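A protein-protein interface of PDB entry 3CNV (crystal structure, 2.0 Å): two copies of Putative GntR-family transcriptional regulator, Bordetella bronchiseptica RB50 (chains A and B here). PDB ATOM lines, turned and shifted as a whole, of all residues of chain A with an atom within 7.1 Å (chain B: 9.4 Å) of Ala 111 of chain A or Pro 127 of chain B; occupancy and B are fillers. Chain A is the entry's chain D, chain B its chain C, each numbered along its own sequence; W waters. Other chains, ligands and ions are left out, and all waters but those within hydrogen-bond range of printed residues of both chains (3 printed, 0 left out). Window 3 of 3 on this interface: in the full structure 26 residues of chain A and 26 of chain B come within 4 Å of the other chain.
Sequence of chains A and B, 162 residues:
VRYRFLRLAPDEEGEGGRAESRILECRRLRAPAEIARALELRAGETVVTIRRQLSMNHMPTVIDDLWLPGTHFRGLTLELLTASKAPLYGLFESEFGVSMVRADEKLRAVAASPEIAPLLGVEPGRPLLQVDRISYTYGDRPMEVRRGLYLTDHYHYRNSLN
The side-chain hydroxyl of Thr 152 of chain B sits at hydrogen-bond distance from the backbone NH of Ala 109 of chain A, 2.9 Å away.
Among the printed residues, merely in contact across the chains: Ala 109 of chain A with Ala 109 of chain B (3.8 Å), Ala 109 of chain A with Leu 128 of chain B (3.3 Å), Ala 109 of chain A with Leu 129 of chain B (3.5 Å), Val 110 of chain A with Pro 127 of chain B (3.6 Å), Ala 111 of chain A with Pro 127 of chain B (3.6 Å), Pro 127 of chain A with Ala 109 of chain B (3.9 Å), Pro 127 of chain A with Val 110 of chain B (3.6 Å), Pro 127 of chain A with Ala 111 of chain B (3.6 Å), Pro 127 of chain A with Pro 127 of chain B (3.9 Å) and Leu 128 of chain A with Ala 109 of chain B (3.3 Å).
The backbone carbonyl oxygen (O) of Leu 129 of chain B sits at hydrogen-bond distance from the backbone NH (N) of Tyr 150 of chain B, 2.9 Å away. The backbone carbonyl oxygen of Val 110 of chain B is in hydrogen-bond range of the backbone NH of Leu 128 of chain B (2.8 Å).
Of chain B, only Pro 127 (3.6 Å) comes within 4 Å of Val 110 of chain A. Ala 111 of chain A touches just one residue of chain B: Pro 127 (3.6 Å). No residue of chain B comes within 4 Å of Ala 112 of chain A. No residue of chain B comes within 4 Å of Gly 125 of chain A. Printed residues of chain B within 4 Å of Pro 127 of chain A: Ala 109, Val 110, Ala 111 and Pro 127. Printed residues of chain B within 4 Å of Leu 128 of chain A: Ala 109 (3.3 Å). Of the printed residues of chain A, Ala 109 of chain B touches Ala 109, Pro 127 and Leu 128. Pro 127 of chain B touches just these residues of chain A: Val 110, Ala 111 and Pro 127. The nearest printed residue of chain B that does not touch Ala 111 of chain A is Arg 126 of chain B (7.1 Å). The nearest residue of chain A that does not touch Pro 127 of chain B is Ala 109 of chain A (4.04 Å). The nearest printed residue of chain B that does not touch Ala 109 of chain A is Pro 127 of chain B (4.04 Å).
Water W2 lies within hydrogen-bond range of the backbone carbonyl oxygen (O) of Ala 109 of chain A (2.4 Å) and the backbone carbonyl oxygen (O) of Thr 152 of chain B (3.3 Å). Water W3 lies within hydrogen-bond range of the backbone carbonyl oxygen (O) of Pro 127 of chain A (2.6 Å) and the backbone carbonyl oxygen (O) of Ala 109 of chain B (3.3 Å).
Of the 25 printed residues of chain B, 7 touch a printed residue of chain A. Printed residues of chain B that touch a printed residue of chain A: Ala 109, Val 110, Ala 111, Pro 127, Leu 128, Leu 129 and Thr 152. Hydrophobic or aromatic side chains of chain B within 4 Å of the printed part of chain A: Ala 109 and Pro 127. Hydrophobic or aromatic side chains of chain A that line the printed part of chain B: Ala 109 and Pro 127. Among the printed residues, no Asp or Glu carboxylate lies within 4 Å of a Lys or Arg side-chain nitrogen of the other chain.
Ala 109 of chain B touches its own counterpart, Ala 109 of chain A. Val 110 of chain A touches Pro 127 of chain B, and with the chains exchanged Pro 127 of chain A touches Val 110 of chain B. Of the 11 pairs that touch across the chains among the printed residues, 8 have their exchanged pair printed and touching as well.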
ATOM      1  N   ALA A 109      -9.824  29.903  -4.766  1.00  0.00           N
ATOM      2  CA  ALA A 109      -8.960  30.608  -3.836  1.00  0.00           C
ATOM      3  C   ALA A 109      -7.560  30.530  -4.388  1.00  0.00           C
ATOM      4  O   ALA A 109      -7.110  29.485  -4.901  1.00  0.00           O
ATOM      5  CB  ALA A 109      -9.050  30.043  -2.416  1.00  0.00           C
ATOM      6  N   VAL A 110      -6.926  31.675  -4.344  1.00  0.00           N
ATOM      7  CA  VAL A 110      -5.598  31.874  -4.973  1.00  0.00           C
ATOM      8  C   VAL A 110      -4.687  32.667  -4.012  1.00  0.00           C
ATOM      9  O   VAL A 110      -5.189  33.389  -3.152  1.00  0.00           O
ATOM     10  CB  VAL A 110      -5.763  32.632  -6.409  1.00  0.00           C
ATOM     11  CG1 VAL A 110      -6.695  31.882  -7.347  1.00  0.00           C
ATOM     12  CG2 VAL A 110      -6.208  34.112  -6.305  1.00  0.00           C
ATOM     13  N   ALA A 111      -3.388  32.527  -4.193  1.00  0.00           N
ATOM     14  CA  ALA A 111      -2.379  33.424  -3.563  1.00  0.00           C
ATOM     15  C   ALA A 111      -2.375  34.821  -4.253  1.00  0.00           C
ATOM     16  O   ALA A 111      -2.350  34.919  -5.474  1.00  0.00           O
ATOM     17  CB  ALA A 111      -0.995  32.823  -3.645  1.00  0.00           C
ATOM     18  N   ALA A 112      -2.360  35.898  -3.470  1.00  0.00           N
ATOM     19  CA  ALA A 112      -2.201  37.244  -4.035  1.00  0.00           C
ATOM     20  C   ALA A 112      -0.930  37.303  -4.841  1.00  0.00           C
ATOM     21  O   ALA A 112       0.146  36.938  -4.344  1.00  0.00           O
ATOM     22  CB  ALA A 112      -2.243  38.341  -2.913  1.00  0.00           C
ATOM     23  N   SER A 113      -1.064  37.652  -6.128  1.00  0.00           N
ATOM     24  CA  SER A 113       0.096  37.789  -7.003  1.00  0.00           C
ATOM     25  C   SER A 113       0.888  39.093  -6.673  1.00  0.00           C
ATOM     26  O   SER A 113       0.337  40.045  -6.073  1.00  0.00           O
ATOM     27  CB  SER A 113      -0.349  37.801  -8.481  1.00  0.00           C
ATOM     28  OG  SER A 113      -1.071  39.009  -8.752  1.00  0.00           O
ATOM     29  N   PRO A 114       2.188  39.147  -7.047  1.00  0.00           N
ATOM     30  CA  PRO A 114       2.958  40.369  -6.911  1.00  0.00           C
ATOM     31  C   PRO A 114       2.273  41.577  -7.535  1.00  0.00           C
ATOM     32  O   PRO A 114       2.399  42.661  -7.054  1.00  0.00           O
ATOM     33  CB  PRO A 114       4.262  40.036  -7.668  1.00  0.00           C
ATOM     34  CG  PRO A 114       4.427  38.564  -7.414  1.00  0.00           C
ATOM     35  CD  PRO A 114       3.034  38.017  -7.475  1.00  0.00           C
ATOM     36  N   ILE A 116      -1.136  42.049  -7.861  1.00  0.00           N
ATOM     37  CA  ILE A 116      -2.417  42.376  -7.237  1.00  0.00           C
ATOM     38  C   ILE A 116      -2.290  42.809  -5.796  1.00  0.00           C
ATOM     39  O   ILE A 116      -2.942  43.728  -5.326  1.00  0.00           O
ATOM     40  CB  ILE A 116      -3.405  41.204  -7.372  1.00  0.00           C
ATOM     41  CG1 ILE A 116      -3.704  40.988  -8.861  1.00  0.00           C
ATOM     42  CG2 ILE A 116      -4.702  41.437  -6.563  1.00  0.00           C
ATOM     43  CD1 ILE A 116      -4.452  42.223  -9.497  1.00  0.00           C
ATOM     44  N   GLU A 123       0.221  41.407   1.539  1.00  0.00           N
ATOM     45  CA  GLU A 123       1.468  40.728   1.156  1.00  0.00           C
ATOM     46  C   GLU A 123       1.181  39.778   0.062  1.00  0.00           C
ATOM     47  O   GLU A 123       0.140  39.049   0.084  1.00  0.00           O
ATOM     48  CB  GLU A 123       2.080  39.924   2.308  1.00  0.00           C
ATOM     49  CG  GLU A 123       1.433  40.250   3.671  1.00  0.00           C
ATOM     50  CD  GLU A 123      -0.035  39.681   3.920  1.00  0.00           C
ATOM     51  OE1 GLU A 123      -0.942  40.513   4.249  1.00  0.00           O
ATOM     52  OE2 GLU A 123      -0.232  38.410   3.847  1.00  0.00           O
ATOM     53  N   PRO A 124       2.061  39.751  -0.938  1.00  0.00           N
ATOM     54  CA  PRO A 124       1.933  38.647  -1.884  1.00  0.00           C
ATOM     55  C   PRO A 124       1.912  37.285  -1.203  1.00  0.00           C
ATOM     56  O   PRO A 124       2.643  37.040  -0.242  1.00  0.00           O
ATOM     57  CB  PRO A 124       3.157  38.799  -2.782  1.00  0.00           C
ATOM     58  CG  PRO A 124       3.660  40.147  -2.569  1.00  0.00           C
ATOM     59  CD  PRO A 124       3.157  40.657  -1.269  1.00  0.00           C
ATOM     60  N   GLY A 125       1.028  36.426  -1.686  1.00  0.00           N
ATOM     61  CA  GLY A 125       0.805  35.137  -1.048  1.00  0.00           C
ATOM     62  C   GLY A 125      -0.496  35.066  -0.247  1.00  0.00           C
ATOM     63  O   GLY A 125      -1.016  33.992   0.007  1.00  0.00           O
ATOM     64  N   ARG A 126      -1.001  36.220   0.147  1.00  0.00           N
ATOM     65  CA  ARG A 126      -2.248  36.326   0.940  1.00  0.00           C
ATOM     66  C   ARG A 126      -3.415  35.638   0.174  1.00  0.00           C
ATOM     67  O   ARG A 126      -3.568  35.870  -1.023  1.00  0.00           O
ATOM     68  CB  ARG A 126      -2.595  37.806   1.192  1.00  0.00           C
ATOM     69  CG  ARG A 126      -3.955  38.072   1.720  1.00  0.00           C
ATOM     70  CD  ARG A 126      -4.051  37.825   3.204  1.00  0.00           C
ATOM     71  NE  ARG A 126      -3.550  38.986   3.900  1.00  0.00           N
ATOM     72  CZ  ARG A 126      -4.291  39.760   4.680  1.00  0.00           C
ATOM     73  NH1 ARG A 126      -5.549  39.428   4.912  1.00  0.00           N
ATOM     74  NH2 ARG A 126      -3.743  40.833   5.234  1.00  0.00           N
ATOM     75  N   PRO A 127      -4.222  34.772   0.840  1.00  0.00           N
ATOM     76  CA  PRO A 127      -5.354  34.165   0.139  1.00  0.00           C
ATOM     77  C   PRO A 127      -6.430  35.190  -0.299  1.00  0.00           C
ATOM     78  O   PRO A 127      -6.840  36.045   0.518  1.00  0.00           O
ATOM     79  CB  PRO A 127      -5.963  33.262   1.186  1.00  0.00           C
ATOM     80  CG  PRO A 127      -4.888  32.985   2.103  1.00  0.00           C
ATOM     81  CD  PRO A 127      -4.058  34.183   2.185  1.00  0.00           C
ATOM     82  N   LEU A 128      -6.771  35.100  -1.585  1.00  0.00           N
ATOM     83  CA  LEU A 128      -7.800  35.908  -2.262  1.00  0.00           C
ATOM     84  C   LEU A 128      -8.845  35.006  -2.901  1.00  0.00           C
ATOM     85  O   LEU A 128      -8.586  33.874  -3.276  1.00  0.00           O
ATOM     86  CB  LEU A 128      -7.204  36.815  -3.325  1.00  0.00           C
ATOM     87  CG  LEU A 128      -6.129  37.816  -2.912  1.00  0.00           C
ATOM     88  CD1 LEU A 128      -5.688  38.659  -4.142  1.00  0.00           C
ATOM     89  CD2 LEU A 128      -6.622  38.716  -1.724  1.00  0.00           C
ATOM     90  N   GLN A 130     -10.770  34.506  -6.111  1.00  0.00           N
ATOM     91  CA  GLN A 130     -10.805  34.842  -7.526  1.00  0.00           C
ATOM     92  C   GLN A 130     -12.174  34.471  -8.130  1.00  0.00           C
ATOM     93  O   GLN A 130     -12.601  33.347  -8.005  1.00  0.00           O
ATOM     94  CB  GLN A 130      -9.722  34.113  -8.258  1.00  0.00           C
ATOM     95  CG  GLN A 130      -9.689  34.486  -9.718  1.00  0.00           C
ATOM     96  CD  GLN A 130      -8.416  33.917 -10.390  1.00  0.00           C
ATOM     97  OE1 GLN A 130      -7.377  34.475 -10.230  1.00  0.00           O
ATOM     98  NE2 GLN A 130      -8.516  32.779 -11.035  1.00  0.00           N
ATOM     99  N   LEU A 149     -10.523  39.765  -8.109  1.00  0.00           N
ATOM    100  CA  LEU A 149      -9.782  39.286  -6.972  1.00  0.00           C
ATOM    101  C   LEU A 149     -10.268  40.048  -5.751  1.00  0.00           C
ATOM    102  O   LEU A 149     -10.138  41.299  -5.681  1.00  0.00           O
ATOM    103  CB  LEU A 149      -8.272  39.486  -7.203  1.00  0.00           C
ATOM    104  CG  LEU A 149      -7.741  38.423  -8.181  1.00  0.00           C
ATOM    105  CD1 LEU A 149      -6.470  38.850  -8.818  1.00  0.00           C
ATOM    106  CD2 LEU A 149      -7.488  37.076  -7.470  1.00  0.00           C
ATOM    107  N   THR B  61      -9.751  16.839  -1.878  1.00  0.00           N
ATOM    108  CA  THR B  61     -10.188  18.094  -2.455  1.00  0.00           C
ATOM    109  C   THR B  61     -11.025  18.948  -1.493  1.00  0.00           C
ATOM    110  O   THR B  61     -10.893  20.179  -1.487  1.00  0.00           O
ATOM    111  CB  THR B  61     -10.958  17.740  -3.777  1.00  0.00           C
ATOM    112  OG1 THR B  61     -10.001  17.180  -4.688  1.00  0.00           O
ATOM    113  CG2 THR B  61     -11.606  18.942  -4.456  1.00  0.00           C
ATOM    114  N   ARG B 108     -15.483  32.516   1.292  1.00  0.00           N
ATOM    115  CA  ARG B 108     -14.254  33.286   1.559  1.00  0.00           C
ATOM    116  C   ARG B 108     -12.997  32.492   1.202  1.00  0.00           C
ATOM    117  O   ARG B 108     -13.030  31.278   1.061  1.00  0.00           O
ATOM    118  CB  ARG B 108     -14.218  33.827   3.012  1.00  0.00           C
ATOM    119  CG  ARG B 108     -14.922  33.010   4.131  1.00  0.00           C
ATOM    120  CD  ARG B 108     -14.869  33.600   5.617  1.00  0.00           C
ATOM    121  NE  ARG B 108     -15.981  34.498   5.983  1.00  0.00           N
ATOM    122  CZ  ARG B 108     -17.209  34.122   6.341  1.00  0.00           C
ATOM    123  NH1 ARG B 108     -17.548  32.867   6.401  1.00  0.00           N
ATOM    124  NH2 ARG B 108     -18.098  35.015   6.661  1.00  0.00           N
ATOM    125  N   ALA B 109     -11.896  33.208   1.025  1.00  0.00           N
ATOM    126  CA  ALA B 109     -10.591  32.553   0.872  1.00  0.00           C
ATOM    127  C   ALA B 109      -9.852  32.673   2.167  1.00  0.00           C
ATOM    128  O   ALA B 109      -9.791  33.755   2.775  1.00  0.00           O
ATOM    129  CB  ALA B 109      -9.730  33.128  -0.297  1.00  0.00           C
ATOM    130  N   VAL B 110      -9.333  31.537   2.582  1.00  0.00           N
ATOM    131  CA  VAL B 110      -8.601  31.417   3.800  1.00  0.00           C
ATOM    132  C   VAL B 110      -7.279  30.670   3.582  1.00  0.00           C
ATOM    133  O   VAL B 110      -7.067  30.057   2.565  1.00  0.00           O
ATOM    134  CB  VAL B 110      -9.481  30.683   4.881  1.00  0.00           C
ATOM    135  CG1 VAL B 110     -10.835  31.446   5.115  1.00  0.00           C
ATOM    136  CG2 VAL B 110      -9.706  29.239   4.548  1.00  0.00           C
ATOM    137  N   ALA B 111      -6.385  30.794   4.554  1.00  0.00           N
ATOM    138  CA  ALA B 111      -5.151  29.962   4.655  1.00  0.00           C
ATOM    139  C   ALA B 111      -5.416  28.608   5.316  1.00  0.00           C
ATOM    140  O   ALA B 111      -6.128  28.499   6.290  1.00  0.00           O
ATOM    141  CB  ALA B 111      -4.030  30.757   5.416  1.00  0.00           C
ATOM    142  N   ALA B 112      -4.884  27.559   4.706  1.00  0.00           N
ATOM    143  CA  ALA B 112      -4.886  26.202   5.284  1.00  0.00           C
ATOM    144  C   ALA B 112      -4.222  26.194   6.641  1.00  0.00           C
ATOM    145  O   ALA B 112      -3.087  26.629   6.816  1.00  0.00           O
ATOM    146  CB  ALA B 112      -4.247  25.192   4.329  1.00  0.00           C
ATOM    147  N   SER B 113      -5.013  25.797   7.623  1.00  0.00           N
ATOM    148  CA  SER B 113      -4.568  25.692   9.020  1.00  0.00           C
ATOM    149  C   SER B 113      -3.626  24.508   9.182  1.00  0.00           C
ATOM    150  O   SER B 113      -3.560  23.582   8.346  1.00  0.00           O
ATOM    151  CB  SER B 113      -5.740  25.526   9.985  1.00  0.00           C
ATOM    152  OG  SER B 113      -6.348  24.253   9.775  1.00  0.00           O
ATOM    153  N   ILE B 116      -5.860  21.347   9.034  1.00  0.00           N
ATOM    154  CA  ILE B 116      -6.460  21.026   7.731  1.00  0.00           C
ATOM    155  C   ILE B 116      -5.445  20.675   6.656  1.00  0.00           C
ATOM    156  O   ILE B 116      -5.655  19.757   5.859  1.00  0.00           O
ATOM    157  CB  ILE B 116      -7.375  22.148   7.252  1.00  0.00           C
ATOM    158  CG1 ILE B 116      -8.545  22.284   8.234  1.00  0.00           C
ATOM    159  CG2 ILE B 116      -7.944  21.912   5.783  1.00  0.00           C
ATOM    160  CD1 ILE B 116      -9.402  21.071   8.305  1.00  0.00           C
ATOM    161  N   ALA B 117      -4.318  21.361   6.673  1.00  0.00           N
ATOM    162  CA  ALA B 117      -3.357  21.245   5.591  1.00  0.00           C
ATOM    163  C   ALA B 117      -3.014  19.762   5.252  1.00  0.00           C
ATOM    164  O   ALA B 117      -3.177  19.353   4.105  1.00  0.00           O
ATOM    165  CB  ALA B 117      -2.124  22.067   5.878  1.00  0.00           C
ATOM    166  N   LEU B 120      -5.526  17.686   3.257  1.00  0.00           N
ATOM    167  CA  LEU B 120      -5.685  18.069   1.838  1.00  0.00           C
ATOM    168  C   LEU B 120      -4.416  17.914   1.036  1.00  0.00           C
ATOM    169  O   LEU B 120      -4.373  18.132  -0.184  1.00  0.00           O
ATOM    170  CB  LEU B 120      -6.244  19.491   1.711  1.00  0.00           C
ATOM    171  CG  LEU B 120      -7.730  19.624   2.117  1.00  0.00           C
ATOM    172  CD1 LEU B 120      -8.191  21.092   2.035  1.00  0.00           C
ATOM    173  CD2 LEU B 120      -8.696  18.739   1.240  1.00  0.00           C
ATOM    174  N   VAL B 122      -1.548  19.497   1.557  1.00  0.00           N
ATOM    175  CA  VAL B 122      -0.893  20.781   1.295  1.00  0.00           C
ATOM    176  C   VAL B 122      -0.147  21.343   2.482  1.00  0.00           C
ATOM    177  O   VAL B 122      -0.257  20.881   3.581  1.00  0.00           O
ATOM    178  CB  VAL B 122      -1.932  21.855   0.836  1.00  0.00           C
ATOM    179  CG1 VAL B 122      -2.689  21.379  -0.400  1.00  0.00           C
ATOM    180  CG2 VAL B 122      -2.960  22.198   1.953  1.00  0.00           C
ATOM    181  N   GLU B 123       0.581  22.406   2.236  1.00  0.00           N
ATOM    182  CA  GLU B 123       1.353  23.067   3.286  1.00  0.00           C
ATOM    183  C   GLU B 123       0.486  24.047   4.055  1.00  0.00           C
ATOM    184  O   GLU B 123      -0.385  24.679   3.493  1.00  0.00           O
ATOM    185  CB  GLU B 123       2.579  23.807   2.685  1.00  0.00           C
ATOM    186  CG  GLU B 123       2.195  25.106   1.962  1.00  0.00           C
ATOM    187  CD  GLU B 123       1.596  24.981   0.501  1.00  0.00           C
ATOM    188  OE1 GLU B 123       1.219  23.835  -0.016  1.00  0.00           O
ATOM    189  OE2 GLU B 123       1.527  26.105  -0.109  1.00  0.00           O
ATOM    190  N   PRO B 124       0.729  24.201   5.357  1.00  0.00           N
ATOM    191  CA  PRO B 124      -0.083  25.242   5.994  1.00  0.00           C
ATOM    192  C   PRO B 124       0.119  26.613   5.355  1.00  0.00           C
ATOM    193  O   PRO B 124       1.225  26.981   4.913  1.00  0.00           O
ATOM    194  CB  PRO B 124       0.399  25.216   7.458  1.00  0.00           C
ATOM    195  CG  PRO B 124       1.070  23.904   7.631  1.00  0.00           C
ATOM    196  CD  PRO B 124       1.663  23.564   6.298  1.00  0.00           C
ATOM    197  N   GLY B 125      -0.945  27.373   5.293  1.00  0.00           N
ATOM    198  CA  GLY B 125      -0.887  28.682   4.630  1.00  0.00           C
ATOM    199  C   GLY B 125      -1.434  28.668   3.222  1.00  0.00           C
ATOM    200  O   GLY B 125      -1.786  29.710   2.676  1.00  0.00           O
ATOM    201  N   ARG B 126      -1.558  27.469   2.654  1.00  0.00           N
ATOM    202  CA  ARG B 126      -2.109  27.286   1.273  1.00  0.00           C
ATOM    203  C   ARG B 126      -3.506  27.891   1.154  1.00  0.00           C
ATOM    204  O   ARG B 126      -4.366  27.685   2.044  1.00  0.00           O
ATOM    205  CB  ARG B 126      -2.176  25.805   0.927  1.00  0.00           C
ATOM    206  CG  ARG B 126      -2.895  25.410  -0.301  1.00  0.00           C
ATOM    207  CD  ARG B 126      -2.202  25.863  -1.550  1.00  0.00           C
ATOM    208  NE  ARG B 126      -1.430  24.772  -2.055  1.00  0.00           N
ATOM    209  CZ  ARG B 126      -1.662  24.142  -3.189  1.00  0.00           C
ATOM    210  NH1 ARG B 126      -2.593  24.541  -4.029  1.00  0.00           N
ATOM    211  NH2 ARG B 126      -0.899  23.144  -3.500  1.00  0.00           N
ATOM    212  N   PRO B 127      -3.742  28.696   0.100  1.00  0.00           N
ATOM    213  CA  PRO B 127      -5.117  29.247   0.050  1.00  0.00           C
ATOM    214  C   PRO B 127      -6.169  28.175  -0.295  1.00  0.00           C
ATOM    215  O   PRO B 127      -5.953  27.307  -1.193  1.00  0.00           O
ATOM    216  CB  PRO B 127      -5.034  30.260  -1.072  1.00  0.00           C
ATOM    217  CG  PRO B 127      -3.658  30.641  -1.169  1.00  0.00           C
ATOM    218  CD  PRO B 127      -2.830  29.405  -0.818  1.00  0.00           C
ATOM    219  N   LEU B 128      -7.252  28.223   0.484  1.00  0.00           N
ATOM    220  CA  LEU B 128      -8.405  27.314   0.347  1.00  0.00           C
ATOM    221  C   LEU B 128      -9.658  28.184   0.245  1.00  0.00           C
ATOM    222  O   LEU B 128      -9.703  29.344   0.754  1.00  0.00           O
ATOM    223  CB  LEU B 128      -8.560  26.381   1.565  1.00  0.00           C
ATOM    224  CG  LEU B 128      -7.365  25.552   1.981  1.00  0.00           C
ATOM    225  CD1 LEU B 128      -7.667  24.747   3.323  1.00  0.00           C
ATOM    226  CD2 LEU B 128      -6.952  24.587   0.832  1.00  0.00           C
ATOM    227  N   LEU B 129     -10.630  27.642  -0.448  1.00  0.00           N
ATOM    228  CA  LEU B 129     -11.988  28.229  -0.581  1.00  0.00           C
ATOM    229  C   LEU B 129     -12.836  27.677   0.571  1.00  0.00           C
ATOM    230  O   LEU B 129     -12.987  26.473   0.748  1.00  0.00           O
ATOM    231  CB  LEU B 129     -12.630  27.922  -1.894  1.00  0.00           C
ATOM    232  CG  LEU B 129     -14.064  28.439  -2.119  1.00  0.00           C
ATOM    233  CD1 LEU B 129     -14.111  29.974  -2.150  1.00  0.00           C
ATOM    234  CD2 LEU B 129     -14.716  27.843  -3.318  1.00  0.00           C
ATOM    235  N   GLN B 130     -13.265  28.585   1.431  1.00  0.00           N
ATOM    236  CA  GLN B 130     -14.148  28.206   2.535  1.00  0.00           C
ATOM    237  C   GLN B 130     -15.585  28.526   2.137  1.00  0.00           C
ATOM    238  O   GLN B 130     -15.927  29.639   1.721  1.00  0.00           O
ATOM    239  CB  GLN B 130     -13.734  28.855   3.852  1.00  0.00           C
ATOM    240  CG  GLN B 130     -14.704  28.622   5.025  1.00  0.00           C
ATOM    241  CD  GLN B 130     -14.154  29.153   6.361  1.00  0.00           C
ATOM    242  OE1 GLN B 130     -13.122  28.710   6.834  1.00  0.00           O
ATOM    243  NE2 GLN B 130     -14.799  30.144   6.907  1.00  0.00           N
ATOM    244  N   LEU B 149     -13.977  23.198   3.252  1.00  0.00           N
ATOM    245  CA  LEU B 149     -12.718  23.792   2.856  1.00  0.00           C
ATOM    246  C   LEU B 149     -12.266  23.022   1.647  1.00  0.00           C
ATOM    247  O   LEU B 149     -12.029  21.821   1.727  1.00  0.00           O
ATOM    248  CB  LEU B 149     -11.674  23.751   4.004  1.00  0.00           C
ATOM    249  CG  LEU B 149     -11.860  24.692   5.203  1.00  0.00           C
ATOM    250  CD1 LEU B 149     -11.043  24.063   6.362  1.00  0.00           C
ATOM    251  CD2 LEU B 149     -11.410  26.180   4.902  1.00  0.00           C
ATOM    252  N   TYR B 150     -12.101  23.769   0.561  1.00  0.00           N
ATOM    253  CA  TYR B 150     -11.871  23.246  -0.756  1.00  0.00           C
ATOM    254  C   TYR B 150     -10.518  23.675  -1.239  1.00  0.00           C
ATOM    255  O   TYR B 150     -10.128  24.845  -1.196  1.00  0.00           O
ATOM    256  CB  TYR B 150     -12.892  23.796  -1.766  1.00  0.00           C
ATOM    257  CG  TYR B 150     -14.347  23.435  -1.552  1.00  0.00           C
ATOM    258  CD1 TYR B 150     -14.968  23.567  -0.318  1.00  0.00           C
ATOM    259  CD2 TYR B 150     -15.121  23.032  -2.607  1.00  0.00           C
ATOM    260  CE1 TYR B 150     -16.348  23.290  -0.157  1.00  0.00           C
ATOM    261  CE2 TYR B 150     -16.513  22.732  -2.456  1.00  0.00           C
ATOM    262  CZ  TYR B 150     -17.101  22.851  -1.214  1.00  0.00           C
ATOM    263  OH  TYR B 150     -18.434  22.575  -1.107  1.00  0.00           O
ATOM    264  N   LEU B 151      -9.801  22.691  -1.743  1.00  0.00           N
ATOM    265  CA  LEU B 151      -8.525  22.946  -2.438  1.00  0.00           C
ATOM    266  C   LEU B 151      -8.897  23.094  -3.928  1.00  0.00           C
ATOM    267  O   LEU B 151      -9.347  22.170  -4.563  1.00  0.00           O
ATOM    268  CB  LEU B 151      -7.569  21.787  -2.258  1.00  0.00           C
ATOM    269  CG  LEU B 151      -6.266  21.886  -3.027  1.00  0.00           C
ATOM    270  CD1 LEU B 151      -5.465  23.079  -2.398  1.00  0.00           C
ATOM    271  CD2 LEU B 151      -5.541  20.550  -2.962  1.00  0.00           C
ATOM    272  N   THR B 152      -8.770  24.308  -4.430  1.00  0.00           N
ATOM    273  CA  THR B 152      -9.246  24.678  -5.760  1.00  0.00           C
ATOM    274  C   THR B 152      -8.131  24.741  -6.784  1.00  0.00           C
ATOM    275  O   THR B 152      -8.126  25.591  -7.653  1.00  0.00           O
ATOM    276  CB  THR B 152     -10.041  26.016  -5.721  1.00  0.00           C
ATOM    277  OG1 THR B 152      -9.224  27.050  -5.192  1.00  0.00           O
ATOM    278  CG2 THR B 152     -11.197  25.892  -4.873  1.00  0.00           C
ATOM    279  N   ASP B 153      -7.190  23.825  -6.703  1.00  0.00           N
ATOM    280  CA  ASP B 153      -6.121  23.828  -7.668  1.00  0.00           C
ATOM    281  C   ASP B 153      -6.460  23.117  -9.012  1.00  0.00           C
ATOM    282  O   ASP B 153      -5.875  23.412 -10.044  1.00  0.00           O
ATOM    283  CB  ASP B 153      -4.748  23.412  -7.031  1.00  0.00           C
ATOM    284  CG  ASP B 153      -4.666  21.945  -6.591  1.00  0.00           C
ATOM    285  OD1 ASP B 153      -3.509  21.403  -6.448  1.00  0.00           O
ATOM    286  OD2 ASP B 153      -5.745  21.348  -6.347  1.00  0.00           O
ATOM    287  N   TYR B 155      -9.891  22.195  -9.514  1.00  0.00           N
ATOM    288  CA  TYR B 155     -11.329  22.296  -9.468  1.00  0.00           C
ATOM    289  C   TYR B 155     -11.688  23.757  -9.049  1.00  0.00           C
ATOM    290  O   TYR B 155     -10.880  24.516  -8.479  1.00  0.00           O
ATOM    291  CB  TYR B 155     -11.921  21.281  -8.498  1.00  0.00           C
ATOM    292  CG  TYR B 155     -11.966  19.826  -8.980  1.00  0.00           C
ATOM    293  CD1 TYR B 155     -13.091  19.317  -9.506  1.00  0.00           C
ATOM    294  CD2 TYR B 155     -10.834  19.001  -8.915  1.00  0.00           C
ATOM    295  CE1 TYR B 155     -13.131  18.010  -9.982  1.00  0.00           C
ATOM    296  CE2 TYR B 155     -10.851  17.698  -9.413  1.00  0.00           C
ATOM    297  CZ  TYR B 155     -12.031  17.214  -9.916  1.00  0.00           C
ATOM    298  OH  TYR B 155     -12.141  15.938 -10.409  1.00  0.00           O
HETATM  299  O   HOH W   1      -7.096  26.483  -3.312  1.00  0.00           O
HETATM  300  O   HOH W   2      -6.223  28.193  -6.774  1.00  0.00           O
HETATM  301  O   HOH W   3      -9.128  36.754   1.462  1.00  0.00           O
